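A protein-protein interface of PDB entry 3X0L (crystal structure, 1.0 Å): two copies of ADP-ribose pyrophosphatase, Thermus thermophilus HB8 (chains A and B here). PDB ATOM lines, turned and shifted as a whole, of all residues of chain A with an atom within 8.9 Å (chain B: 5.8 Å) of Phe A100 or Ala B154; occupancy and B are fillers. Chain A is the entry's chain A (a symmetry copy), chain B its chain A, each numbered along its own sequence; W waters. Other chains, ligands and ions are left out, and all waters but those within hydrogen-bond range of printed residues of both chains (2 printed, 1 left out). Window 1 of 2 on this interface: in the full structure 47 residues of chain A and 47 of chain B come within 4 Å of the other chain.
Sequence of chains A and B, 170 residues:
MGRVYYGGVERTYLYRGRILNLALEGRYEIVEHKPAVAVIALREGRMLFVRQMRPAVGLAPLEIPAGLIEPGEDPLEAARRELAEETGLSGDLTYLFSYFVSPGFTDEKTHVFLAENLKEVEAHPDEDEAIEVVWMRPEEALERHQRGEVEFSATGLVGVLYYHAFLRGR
Hydrophobic or aromatic side chains of chain B that line the printed part of chain A: Val B57, Leu B59, Pro B61, Tyr B99, Phe B152, Ala B154, Leu B157 and Val B158.
Along chain B the printed residues that touch a printed residue of chain A span positions 57 to 158.
Printed residues of chain A that touch a printed residue of chain B: Phe A97, Ser A98, Tyr A99, Phe A100, Val A101, Pro A103, Thr A106, Asp A107, Lys A109, Ser A153, Ala A154, Leu A157 and Leu A161.
Among the printed residues, 23 pairs touch across the chains.
Among the printed residues, merely in contact across the chains: Phe A97 with Leu B157, Ser A98 with Glu B151, Ser A98 with Phe B152, Tyr A99 with Phe B152, Tyr A99 with Ser B153, Tyr A99 with Ala B154, Tyr A99 with Leu B157, Phe A100 with Val B57, Phe A100 with Leu B59, Phe A100 with Glu B151, Phe A100 with Ser B153, Val A101 with Ala B154, Pro A103 with Pro B61, Pro A103 with Ser B153, Thr A106 with Val B57, Asp A107 with Val B57, Ser A153 with Tyr B99, Ala A154 with Tyr B99, Leu A157 with Tyr B99 and Leu A161 with Val B158.
OG of Ser B153 is in hydrogen-bond range of N of Gly B156 (3.0 Å).
N of His A33 is in hydrogen-bond range of OD2 of Asp A107, at 2.8 Å.
O of Phe A97 is in hydrogen-bond range of N of Val A112.
O of Tyr A99 lies within hydrogen-bond range of N of Thr A110.
N of Val A101 is in hydrogen-bond range of O of Glu A108, 3.0 Å away.
The side-chain hydroxyl (OG1) of Thr A106 lies within hydrogen-bond range of the backbone NH (N) of Glu A108, 3.2 Å away.
Of the printed residues of chain B, Phe A97 touches Leu B157 (3.8 Å).
Of the printed residues of chain B, Ser A98 touches Glu B151 (3.9 Å) and Phe B152 (3.8 Å).
Of the printed residues of chain B, Phe A100 touches Val B57 (3.5 Å), Leu B59 (3.96 Å), Glu B151 (3.8 Å), Phe B152 (2.9 Å), Ser B153 (3.5 Å) and Ala B154 (2.8 Å).
Glu A108 touches none of the printed residues of chain B.
Of the printed residues of chain B, Ala A154 touches Tyr B99 (3.6 Å).
Printed residues of chain B within 4 Å of Leu A161: Val B158.
Ala B154 touches just these residues of chain A: Tyr A99 (3.6 Å), Phe A100 (2.8 Å) and Val A101 (3.7 Å).
No residue of chain A comes within 4 Å of Thr B155.
Gly B156 touches none of the printed residues of chain A.
The nearest residue of chain B that does not touch Phe A100 is Pro B61 (4.3 Å).
The nearest residue of chain A that does not touch Ala B154 is Ala A154 (4.9 Å).
The nearest printed residue of chain A that does not touch Val B158 is Leu A157 (4.1 Å).
Tyr A99 touches Ser B153, and with the chains exchanged Ser A153 touches Tyr B99.
Tyr A99 touches Ala B154, and with the chains exchanged Ala A154 touches Tyr B99.
Tyr A99 touches Leu B157, and with the chains exchanged Leu A157 touches Tyr B99.
Of the 23 pairs that touch across the chains among the printed residues, 6 have their exchanged pair printed and touching as well.
Water W1 lies within hydrogen-bond range of the side-chain carboxylate (OE1) of Glu B151, the backbone NH (N) of Phe B152 and the side-chain hydroxyl (OG) of Ser A98.
Water W2 bridges O of Val A101 (2.8 Å) and OH of Tyr B99 (2.8 Å).
The side-chain carboxylate (OE1) of Glu B151 is in salt-bridge range of the side-chain amino group (NZ) of Lys A109 (3.0 Å).
The backbone carbonyl oxygen (O) of Phe B152 is in hydrogen-bond range of the backbone NH (N) of Phe A100 (2.9 Å).
The backbone carbonyl oxygen (O) of Phe A100 sits at hydrogen-bond distance from the backbone NH (N) of Ala B154 (2.8 Å).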
ATOM      1  N   HIS A  33     -17.348 -18.688  -1.189  1.00  0.00           N
ATOM      2  CA  HIS A  33     -17.811 -18.265  -2.513  1.00  0.00           C
ATOM      3  C   HIS A  33     -17.444 -19.298  -3.537  1.00  0.00           C
ATOM      4  O   HIS A  33     -16.366 -19.910  -3.451  1.00  0.00           O
ATOM      5  CB  HIS A  33     -17.079 -16.947  -2.803  1.00  0.00           C
ATOM      6  CG  HIS A  33     -17.509 -16.190  -4.035  1.00  0.00           C
ATOM      7  ND1 HIS A  33     -17.309 -16.662  -5.336  1.00  0.00           N
ATOM      8  CD2 HIS A  33     -18.082 -14.973  -4.142  1.00  0.00           C
ATOM      9  CE1 HIS A  33     -17.745 -15.725  -6.178  1.00  0.00           C
ATOM     10  NE2 HIS A  33     -18.238 -14.692  -5.497  1.00  0.00           N
ATOM     11  N   PRO A  35     -15.938 -21.062  -6.833  1.00  0.00           N
ATOM     12  CA  PRO A  35     -14.767 -20.710  -7.646  1.00  0.00           C
ATOM     13  C   PRO A  35     -15.182 -20.045  -8.957  1.00  0.00           C
ATOM     14  O   PRO A  35     -16.316 -20.205  -9.446  1.00  0.00           O
ATOM     15  CB  PRO A  35     -14.008 -22.022  -7.815  1.00  0.00           C
ATOM     16  CG  PRO A  35     -15.049 -23.076  -7.640  1.00  0.00           C
ATOM     17  CD  PRO A  35     -16.096 -22.525  -6.729  1.00  0.00           C
ATOM     18  N   PHE A  97      -2.837 -20.471 -14.528  1.00  0.00           N
ATOM     19  CA  PHE A  97      -2.530 -20.352 -13.087  1.00  0.00           C
ATOM     20  C   PHE A  97      -3.854 -20.017 -12.400  1.00  0.00           C
ATOM     21  O   PHE A  97      -4.872 -19.714 -13.063  1.00  0.00           O
ATOM     22  CB  PHE A  97      -1.450 -19.294 -12.779  1.00  0.00           C
ATOM     23  CG  PHE A  97      -1.506 -18.040 -13.619  1.00  0.00           C
ATOM     24  CD1 PHE A  97      -0.387 -17.728 -14.421  1.00  0.00           C
ATOM     25  CD2 PHE A  97      -2.606 -17.192 -13.599  1.00  0.00           C
ATOM     26  CE1 PHE A  97      -0.398 -16.589 -15.233  1.00  0.00           C
ATOM     27  CE2 PHE A  97      -2.640 -16.057 -14.418  1.00  0.00           C
ATOM     28  CZ  PHE A  97      -1.515 -15.756 -15.235  1.00  0.00           C
ATOM     29  N   SER A  98      -3.811 -20.082 -11.078  1.00  0.00           N
ATOM     30  CA  SER A  98      -4.966 -19.741 -10.261  1.00  0.00           C
ATOM     31  C   SER A  98      -4.531 -18.800  -9.149  1.00  0.00           C
ATOM     32  O   SER A  98      -3.339 -18.698  -8.818  1.00  0.00           O
ATOM     33  CB  SER A  98      -5.569 -21.005  -9.647  1.00  0.00           C
ATOM     34  OG  SER A  98      -4.645 -21.528  -8.693  1.00  0.00           O
ATOM     35  N   TYR A  99      -5.531 -18.154  -8.538  1.00  0.00           N
ATOM     36  CA  TYR A  99      -5.218 -17.297  -7.392  1.00  0.00           C
ATOM     37  C   TYR A  99      -6.451 -17.182  -6.513  1.00  0.00           C
ATOM     38  O   TYR A  99      -7.591 -17.226  -6.972  1.00  0.00           O
ATOM     39  CB  TYR A  99      -4.737 -15.902  -7.806  1.00  0.00           C
ATOM     40  CG  TYR A  99      -5.757 -15.063  -8.556  1.00  0.00           C
ATOM     41  CD1 TYR A  99      -5.935 -15.170  -9.942  1.00  0.00           C
ATOM     42  CD2 TYR A  99      -6.586 -14.165  -7.864  1.00  0.00           C
ATOM     43  CE1 TYR A  99      -6.877 -14.400 -10.590  1.00  0.00           C
ATOM     44  CE2 TYR A  99      -7.529 -13.396  -8.523  1.00  0.00           C
ATOM     45  CZ  TYR A  99      -7.690 -13.498  -9.886  1.00  0.00           C
ATOM     46  OH  TYR A  99      -8.608 -12.785 -10.594  1.00  0.00           O
ATOM     47  N   PHE A 100      -6.186 -16.983  -5.217  1.00  0.00           N
ATOM     48  CA  PHE A 100      -7.250 -16.615  -4.262  1.00  0.00           C
ATOM     49  C   PHE A 100      -7.420 -15.120  -4.304  1.00  0.00           C
ATOM     50  O   PHE A 100      -6.466 -14.349  -4.114  1.00  0.00           O
ATOM     51  CB  PHE A 100      -6.825 -17.055  -2.849  1.00  0.00           C
ATOM     52  CG  PHE A 100      -6.891 -18.554  -2.672  1.00  0.00           C
ATOM     53  CD1 PHE A 100      -5.766 -19.298  -2.497  1.00  0.00           C
ATOM     54  CD2 PHE A 100      -8.145 -19.201  -2.659  1.00  0.00           C
ATOM     55  CE1 PHE A 100      -5.886 -20.671  -2.261  1.00  0.00           C
ATOM     56  CE2 PHE A 100      -8.241 -20.562  -2.467  1.00  0.00           C
ATOM     57  CZ  PHE A 100      -7.104 -21.296  -2.256  1.00  0.00           C
ATOM     58  N   VAL A 101      -8.668 -14.653  -4.550  1.00  0.00           N
ATOM     59  CA  VAL A 101      -8.901 -13.241  -4.780  1.00  0.00           C
ATOM     60  C   VAL A 101      -8.542 -12.382  -3.554  1.00  0.00           C
ATOM     61  O   VAL A 101      -8.108 -11.238  -3.747  1.00  0.00           O
ATOM     62  CB  VAL A 101     -10.340 -12.929  -5.236  1.00  0.00           C
ATOM     63  CG1 VAL A 101     -10.736 -13.842  -6.402  1.00  0.00           C
ATOM     64  CG2 VAL A 101     -11.351 -13.025  -4.101  1.00  0.00           C
ATOM     65  N   SER A 102      -8.795 -12.903  -2.356  1.00  0.00           N
ATOM     66  CA  SER A 102      -8.575 -12.106  -1.143  1.00  0.00           C
ATOM     67  C   SER A 102      -8.652 -13.053   0.046  1.00  0.00           C
ATOM     68  O   SER A 102      -9.659 -13.134   0.740  1.00  0.00           O
ATOM     69  CB  SER A 102      -9.601 -10.967  -1.020  1.00  0.00           C
ATOM     70  OG  SER A 102      -9.176 -10.112  -0.003  1.00  0.00           O
ATOM     71  N   PRO A 103      -7.590 -13.836   0.267  1.00  0.00           N
ATOM     72  CA  PRO A 103      -7.668 -14.966   1.195  1.00  0.00           C
ATOM     73  C   PRO A 103      -7.701 -14.558   2.653  1.00  0.00           C
ATOM     74  O   PRO A 103      -7.889 -15.448   3.500  1.00  0.00           O
ATOM     75  CB  PRO A 103      -6.443 -15.806   0.870  1.00  0.00           C
ATOM     76  CG  PRO A 103      -5.441 -14.783   0.333  1.00  0.00           C
ATOM     77  CD  PRO A 103      -6.301 -13.820  -0.469  1.00  0.00           C
ATOM     78  N   GLY A 104      -7.600 -13.259   2.972  1.00  0.00           N
ATOM     79  CA  GLY A 104      -7.865 -12.811   4.335  1.00  0.00           C
ATOM     80  C   GLY A 104      -9.333 -12.867   4.736  1.00  0.00           C
ATOM     81  O   GLY A 104      -9.595 -12.815   5.936  1.00  0.00           O
ATOM     82  N   PHE A 105     -10.251 -13.005   3.769  1.00  0.00           N
ATOM     83  CA  PHE A 105     -11.664 -13.118   4.177  1.00  0.00           C
ATOM     84  C   PHE A 105     -12.483 -14.054   3.327  1.00  0.00           C
ATOM     85  O   PHE A 105     -13.552 -14.451   3.811  1.00  0.00           O
ATOM     86  CB  PHE A 105     -12.346 -11.751   4.286  1.00  0.00           C
ATOM     87  CG  PHE A 105     -12.911 -11.228   2.982  1.00  0.00           C
ATOM     88  CD1 PHE A 105     -14.267 -11.356   2.708  1.00  0.00           C
ATOM     89  CD2 PHE A 105     -12.085 -10.613   2.039  1.00  0.00           C
ATOM     90  CE1 PHE A 105     -14.820 -10.940   1.517  1.00  0.00           C
ATOM     91  CE2 PHE A 105     -12.648 -10.164   0.849  1.00  0.00           C
ATOM     92  CZ  PHE A 105     -14.030 -10.308   0.592  1.00  0.00           C
ATOM     93  N   THR A 106     -12.067 -14.375   2.104  1.00  0.00           N
ATOM     94  CA  THR A 106     -12.895 -15.229   1.284  1.00  0.00           C
ATOM     95  C   THR A 106     -12.074 -16.368   0.742  1.00  0.00           C
ATOM     96  O   THR A 106     -10.848 -16.272   0.556  1.00  0.00           O
ATOM     97  CB  THR A 106     -13.601 -14.427   0.151  1.00  0.00           C
ATOM     98  OG1 THR A 106     -14.444 -15.314  -0.606  1.00  0.00           O
ATOM     99  CG2 THR A 106     -12.619 -13.788  -0.836  1.00  0.00           C
ATOM    100  N   ASP A 107     -12.756 -17.472   0.405  1.00  0.00           N
ATOM    101  CA  ASP A 107     -12.112 -18.606  -0.220  1.00  0.00           C
ATOM    102  C   ASP A 107     -12.270 -18.572  -1.747  1.00  0.00           C
ATOM    103  O   ASP A 107     -11.852 -19.531  -2.418  1.00  0.00           O
ATOM    104  CB  ASP A 107     -12.567 -19.951   0.315  1.00  0.00           C
ATOM    105  CG  ASP A 107     -14.062 -20.154   0.102  1.00  0.00           C
ATOM    106  OD1 ASP A 107     -14.584 -21.167   0.632  1.00  0.00           O
ATOM    107  OD2 ASP A 107     -14.699 -19.349  -0.597  1.00  0.00           O
ATOM    108  N   GLU A 108     -12.778 -17.466  -2.344  1.00  0.00           N
ATOM    109  CA  GLU A 108     -12.934 -17.489  -3.801  1.00  0.00           C
ATOM    110  C   GLU A 108     -11.584 -17.692  -4.482  1.00  0.00           C
ATOM    111  O   GLU A 108     -10.638 -16.940  -4.224  1.00  0.00           O
ATOM    112  CB  GLU A 108     -13.547 -16.165  -4.306  1.00  0.00           C
ATOM    113  CG  GLU A 108     -13.851 -16.241  -5.795  1.00  0.00           C
ATOM    114  CD  GLU A 108     -14.400 -14.954  -6.373  1.00  0.00           C
ATOM    115  OE1 GLU A 108     -14.337 -13.930  -5.746  1.00  0.00           O
ATOM    116  OE2 GLU A 108     -14.883 -15.018  -7.523  1.00  0.00           O
ATOM    117  N   LYS A 109     -11.558 -18.667  -5.386  1.00  0.00           N
ATOM    118  CA  LYS A 109     -10.371 -19.028  -6.140  1.00  0.00           C
ATOM    119  C   LYS A 109     -10.721 -18.838  -7.625  1.00  0.00           C
ATOM    120  O   LYS A 109     -11.771 -19.307  -8.050  1.00  0.00           O
ATOM    121  CB  LYS A 109      -9.950 -20.445  -5.844  1.00  0.00           C
ATOM    122  CG  LYS A 109      -8.622 -20.829  -6.470  1.00  0.00           C
ATOM    123  CD  LYS A 109      -8.207 -22.278  -6.089  1.00  0.00           C
ATOM    124  CE  LYS A 109      -6.687 -22.426  -6.084  1.00  0.00           C
ATOM    125  NZ  LYS A 109      -6.409 -23.909  -5.862  1.00  0.00           N
ATOM    126  N   THR A 110      -9.831 -18.182  -8.357  1.00  0.00           N
ATOM    127  CA  THR A 110     -10.031 -17.928  -9.786  1.00  0.00           C
ATOM    128  C   THR A 110      -8.990 -18.700 -10.590  1.00  0.00           C
ATOM    129  O   THR A 110      -7.797 -18.629 -10.305  1.00  0.00           O
ATOM    130  CB  THR A 110      -9.874 -16.426 -10.063  1.00  0.00           C
ATOM    131  OG1 THR A 110     -10.826 -15.730  -9.239  1.00  0.00           O
ATOM    132  CG2 THR A 110     -10.171 -16.084 -11.490  1.00  0.00           C
ATOM    133  N   HIS A 111      -9.481 -19.399 -11.618  1.00  0.00           N
ATOM    134  CA  HIS A 111      -8.655 -20.179 -12.501  1.00  0.00           C
ATOM    135  C   HIS A 111      -8.555 -19.433 -13.860  1.00  0.00           C
ATOM    136  O   HIS A 111      -9.608 -19.150 -14.457  1.00  0.00           O
ATOM    137  CB  HIS A 111      -9.279 -21.552 -12.745  1.00  0.00           C
ATOM    138  CG  HIS A 111      -9.507 -22.317 -11.479  1.00  0.00           C
ATOM    139  ND1 HIS A 111      -8.592 -23.156 -10.987  1.00  0.00           N
ATOM    140  CD2 HIS A 111     -10.537 -22.257 -10.616  1.00  0.00           C
ATOM    141  CE1 HIS A 111      -9.050 -23.705  -9.848  1.00  0.00           C
ATOM    142  NE2 HIS A 111     -10.243 -23.176  -9.618  1.00  0.00           N
ATOM    143  N   VAL A 112      -7.341 -19.121 -14.275  1.00  0.00           N
ATOM    144  CA  VAL A 112      -7.140 -18.258 -15.434  1.00  0.00           C
ATOM    145  C   VAL A 112      -6.632 -19.086 -16.634  1.00  0.00           C
ATOM    146  O   VAL A 112      -5.710 -19.900 -16.477  1.00  0.00           O
ATOM    147  CB  VAL A 112      -6.133 -17.128 -15.094  1.00  0.00           C
ATOM    148  CG1 VAL A 112      -6.064 -16.166 -16.295  1.00  0.00           C
ATOM    149  CG2 VAL A 112      -6.565 -16.400 -13.853  1.00  0.00           C
ATOM    150  N   SER A 153     -10.653  -4.682 -12.546  1.00  0.00           N
ATOM    151  CA  SER A 153     -10.822  -5.824 -11.645  1.00  0.00           C
ATOM    152  C   SER A 153      -9.474  -6.556 -11.561  1.00  0.00           C
ATOM    153  O   SER A 153      -8.592  -6.366 -12.414  1.00  0.00           O
ATOM    154  CB  SER A 153     -11.869  -6.798 -12.142  1.00  0.00           C
ATOM    155  OG  SER A 153     -11.434  -7.390 -13.367  1.00  0.00           O
ATOM    156  N   ALA A 154      -9.352  -7.455 -10.595  1.00  0.00           N
ATOM    157  CA  ALA A 154      -8.178  -8.322 -10.550  1.00  0.00           C
ATOM    158  C   ALA A 154      -8.014  -9.060 -11.870  1.00  0.00           C
ATOM    159  O   ALA A 154      -6.891  -9.188 -12.366  1.00  0.00           O
ATOM    160  CB  ALA A 154      -8.281  -9.309  -9.402  1.00  0.00           C
ATOM    161  N   THR A 155      -9.105  -9.572 -12.436  1.00  0.00           N
ATOM    162  CA  THR A 155      -8.934 -10.336 -13.680  1.00  0.00           C
ATOM    163  C   THR A 155      -8.409  -9.459 -14.801  1.00  0.00           C
ATOM    164  O   THR A 155      -7.561  -9.868 -15.597  1.00  0.00           O
ATOM    165  CB  THR A 155     -10.233 -11.052 -14.099  1.00  0.00           C
ATOM    166  OG1 THR A 155     -11.268 -10.076 -14.300  1.00  0.00           O
ATOM    167  CG2 THR A 155     -10.666 -12.109 -13.067  1.00  0.00           C
ATOM    168  N   LEU A 157      -6.542  -6.673 -14.521  1.00  0.00           N
ATOM    169  CA  LEU A 157      -5.152  -6.361 -14.252  1.00  0.00           C
ATOM    170  C   LEU A 157      -4.254  -7.573 -14.520  1.00  0.00           C
ATOM    171  O   LEU A 157      -3.180  -7.420 -15.128  1.00  0.00           O
ATOM    172  CB  LEU A 157      -5.008  -5.886 -12.809  1.00  0.00           C
ATOM    173  CG  LEU A 157      -3.558  -5.591 -12.372  1.00  0.00           C
ATOM    174  CD1 LEU A 157      -2.955  -4.441 -13.166  1.00  0.00           C
ATOM    175  CD2 LEU A 157      -3.553  -5.269 -10.876  1.00  0.00           C
ATOM    176  N   VAL A 158      -4.675  -8.746 -14.094  1.00  0.00           N
ATOM    177  CA  VAL A 158      -3.899  -9.972 -14.384  1.00  0.00           C
ATOM    178  C   VAL A 158      -3.764 -10.142 -15.866  1.00  0.00           C
ATOM    179  O   VAL A 158      -2.668 -10.482 -16.361  1.00  0.00           O
ATOM    180  CB  VAL A 158      -4.581 -11.189 -13.701  1.00  0.00           C
ATOM    181  CG1 VAL A 158      -4.075 -12.489 -14.287  1.00  0.00           C
ATOM    182  CG2 VAL A 158      -4.340 -11.106 -12.197  1.00  0.00           C
ATOM    183  N   LEU A 161      -1.141  -7.582 -17.127  1.00  0.00           N
ATOM    184  CA  LEU A 161       0.233  -7.916 -16.717  1.00  0.00           C
ATOM    185  C   LEU A 161       0.749  -9.161 -17.397  1.00  0.00           C
ATOM    186  O   LEU A 161       1.913  -9.205 -17.811  1.00  0.00           O
ATOM    187  CB  LEU A 161       0.340  -8.028 -15.194  1.00  0.00           C
ATOM    188  CG  LEU A 161       0.003  -6.745 -14.427  1.00  0.00           C
ATOM    189  CD1 LEU A 161       0.037  -7.015 -12.917  1.00  0.00           C
ATOM    190  CD2 LEU A 161       0.979  -5.612 -14.783  1.00  0.00           C
ATOM    191  N   VAL B  57      -9.122 -20.032   3.786  1.00  0.00           N
ATOM    192  CA  VAL B  57      -8.739 -21.068   2.808  1.00  0.00           C
ATOM    193  C   VAL B  57      -8.084 -22.249   3.424  1.00  0.00           C
ATOM    194  O   VAL B  57      -7.879 -23.261   2.740  1.00  0.00           O
ATOM    195  CB  VAL B  57      -7.879 -20.473   1.651  1.00  0.00           C
ATOM    196  CG1 VAL B  57      -8.735 -19.510   0.856  1.00  0.00           C
ATOM    197  CG2 VAL B  57      -6.642 -19.781   2.162  1.00  0.00           C
ATOM    198  N   LEU B  59      -5.038 -22.706   4.461  1.00  0.00           N
ATOM    199  CA  LEU B  59      -3.670 -22.883   3.991  1.00  0.00           C
ATOM    200  C   LEU B  59      -2.993 -21.517   3.959  1.00  0.00           C
ATOM    201  O   LEU B  59      -3.652 -20.517   4.232  1.00  0.00           O
ATOM    202  CB  LEU B  59      -3.655 -23.646   2.638  1.00  0.00           C
ATOM    203  CG  LEU B  59      -4.439 -23.009   1.494  1.00  0.00           C
ATOM    204  CD1 LEU B  59      -3.665 -21.939   0.757  1.00  0.00           C
ATOM    205  CD2 LEU B  59      -4.832 -24.070   0.447  1.00  0.00           C
ATOM    206  N   PRO B  61      -1.216 -19.207   1.466  1.00  0.00           N
ATOM    207  CA  PRO B  61      -0.826 -18.929   0.068  1.00  0.00           C
ATOM    208  C   PRO B  61       0.384 -18.009   0.026  1.00  0.00           C
ATOM    209  O   PRO B  61       0.760 -17.353   1.007  1.00  0.00           O
ATOM    210  CB  PRO B  61      -2.059 -18.230  -0.514  1.00  0.00           C
ATOM    211  CG  PRO B  61      -2.833 -17.758   0.629  1.00  0.00           C
ATOM    212  CD  PRO B  61      -2.441 -18.488   1.878  1.00  0.00           C
ATOM    213  N   TYR B  99      -6.749  -2.317  -8.014  1.00  0.00           N
ATOM    214  CA  TYR B  99      -7.714  -3.242  -8.613  1.00  0.00           C
ATOM    215  C   TYR B  99      -8.764  -3.596  -7.577  1.00  0.00           C
ATOM    216  O   TYR B  99      -8.511  -3.645  -6.374  1.00  0.00           O
ATOM    217  CB  TYR B  99      -7.058  -4.518  -9.153  1.00  0.00           C
ATOM    218  CG  TYR B  99      -6.392  -5.394  -8.106  1.00  0.00           C
ATOM    219  CD1 TYR B  99      -5.078  -5.169  -7.673  1.00  0.00           C
ATOM    220  CD2 TYR B  99      -7.097  -6.453  -7.510  1.00  0.00           C
ATOM    221  CE1 TYR B  99      -4.508  -5.978  -6.713  1.00  0.00           C
ATOM    222  CE2 TYR B  99      -6.515  -7.260  -6.549  1.00  0.00           C
ATOM    223  CZ  TYR B  99      -5.222  -7.039  -6.136  1.00  0.00           C
ATOM    224  OH  TYR B  99      -4.594  -7.783  -5.184  1.00  0.00           O
ATOM    225  N   GLU B 151       0.071 -22.164  -3.616  1.00  0.00           N
ATOM    226  CA  GLU B 151      -1.056 -21.389  -4.093  1.00  0.00           C
ATOM    227  C   GLU B 151      -0.667 -19.910  -4.048  1.00  0.00           C
ATOM    228  O   GLU B 151       0.179 -19.509  -3.272  1.00  0.00           O
ATOM    229  CB  GLU B 151      -2.273 -21.600  -3.194  1.00  0.00           C
ATOM    230  CG  GLU B 151      -2.669 -23.065  -2.994  1.00  0.00           C
ATOM    231  CD  GLU B 151      -3.125 -23.685  -4.265  1.00  0.00           C
ATOM    232  OE1 GLU B 151      -3.641 -23.024  -5.197  1.00  0.00           O
ATOM    233  OE2 GLU B 151      -3.045 -24.929  -4.464  1.00  0.00           O
ATOM    234  N   PHE B 152      -1.302 -19.114  -4.918  1.00  0.00           N
ATOM    235  CA  PHE B 152      -1.111 -17.670  -4.926  1.00  0.00           C
ATOM    236  C   PHE B 152      -2.287 -16.951  -4.330  1.00  0.00           C
ATOM    237  O   PHE B 152      -3.431 -17.370  -4.568  1.00  0.00           O
ATOM    238  CB  PHE B 152      -0.972 -17.127  -6.352  1.00  0.00           C
ATOM    239  CG  PHE B 152       0.392 -17.262  -6.985  1.00  0.00           C
ATOM    240  CD1 PHE B 152       0.516 -17.929  -8.220  1.00  0.00           C
ATOM    241  CD2 PHE B 152       1.480 -16.650  -6.421  1.00  0.00           C
ATOM    242  CE1 PHE B 152       1.770 -18.005  -8.835  1.00  0.00           C
ATOM    243  CE2 PHE B 152       2.720 -16.726  -7.022  1.00  0.00           C
ATOM    244  CZ  PHE B 152       2.879 -17.369  -8.230  1.00  0.00           C
ATOM    245  N   SER B 153      -2.036 -15.831  -3.663  1.00  0.00           N
ATOM    246  CA  SER B 153      -3.086 -14.818  -3.541  1.00  0.00           C
ATOM    247  C   SER B 153      -3.032 -13.939  -4.801  1.00  0.00           C
ATOM    248  O   SER B 153      -2.027 -13.931  -5.530  1.00  0.00           O
ATOM    249  CB  SER B 153      -2.893 -13.932  -2.329  1.00  0.00           C
ATOM    250  OG  SER B 153      -1.694 -13.169  -2.473  1.00  0.00           O
ATOM    251  N   ALA B 154      -4.067 -13.135  -5.002  1.00  0.00           N
ATOM    252  CA  ALA B 154      -4.021 -12.140  -6.070  1.00  0.00           C
ATOM    253  C   ALA B 154      -2.792 -11.257  -5.917  1.00  0.00           C
ATOM    254  O   ALA B 154      -2.136 -10.942  -6.914  1.00  0.00           O
ATOM    255  CB  ALA B 154      -5.282 -11.296  -6.074  1.00  0.00           C
ATOM    256  N   THR B 155      -2.483 -10.827  -4.696  1.00  0.00           N
ATOM    257  CA  THR B 155      -1.330  -9.924  -4.562  1.00  0.00           C
ATOM    258  C   THR B 155      -0.040 -10.611  -4.964  1.00  0.00           C
ATOM    259  O   THR B 155       0.831 -10.022  -5.609  1.00  0.00           O
ATOM    260  CB  THR B 155      -1.224  -9.332  -3.142  1.00  0.00           C
ATOM    261  OG1 THR B 155      -1.082 -10.403  -2.193  1.00  0.00           O
ATOM    262  CG2 THR B 155      -2.435  -8.448  -2.796  1.00  0.00           C
ATOM    263  N   GLY B 156       0.128 -11.901  -4.562  1.00  0.00           N
ATOM    264  CA  GLY B 156       1.327 -12.623  -4.977  1.00  0.00           C
ATOM    265  C   GLY B 156       1.439 -12.786  -6.471  1.00  0.00           C
ATOM    266  O   GLY B 156       2.530 -12.606  -7.057  1.00  0.00           O
ATOM    267  N   LEU B 157       0.338 -13.161  -7.127  1.00  0.00           N
ATOM    268  CA  LEU B 157       0.345 -13.328  -8.566  1.00  0.00           C
ATOM    269  C   LEU B 157       0.610 -11.995  -9.273  1.00  0.00           C
ATOM    270  O   LEU B 157       1.402 -11.952 -10.231  1.00  0.00           O
ATOM    271  CB  LEU B 157      -0.985 -13.927  -9.015  1.00  0.00           C
ATOM    272  CG  LEU B 157      -1.135 -14.086 -10.543  1.00  0.00           C
ATOM    273  CD1 LEU B 157      -0.117 -15.066 -11.108  1.00  0.00           C
ATOM    274  CD2 LEU B 157      -2.558 -14.557 -10.849  1.00  0.00           C
ATOM    275  N   VAL B 158      -0.021 -10.931  -8.818  1.00  0.00           N
ATOM    276  CA  VAL B 158       0.242  -9.596  -9.399  1.00  0.00           C
ATOM    277  C   VAL B 158       1.694  -9.260  -9.248  1.00  0.00           C
ATOM    278  O   VAL B 158       2.319  -8.740 -10.197  1.00  0.00           O
ATOM    279  CB  VAL B 158      -0.689  -8.548  -8.730  1.00  0.00           C
ATOM    280  CG1 VAL B 158      -0.190  -7.142  -8.986  1.00  0.00           C
ATOM    281  CG2 VAL B 158      -2.110  -8.754  -9.244  1.00  0.00           C
ATOM    282  N   GLY B 159       2.312  -9.534  -8.096  1.00  0.00           N
ATOM    283  CA  GLY B 159       3.742  -9.228  -7.945  1.00  0.00           C
ATOM    284  C   GLY B 159       4.572 -10.009  -8.948  1.00  0.00           C
ATOM    285  O   GLY B 159       5.474  -9.458  -9.593  1.00  0.00           O
HETATM  286  O   HOH W   1      -3.448 -20.498  -6.209  1.00  0.00           O
HETATM  287  O   HOH W   2      -6.145  -9.279  -3.364  1.00  0.00           O
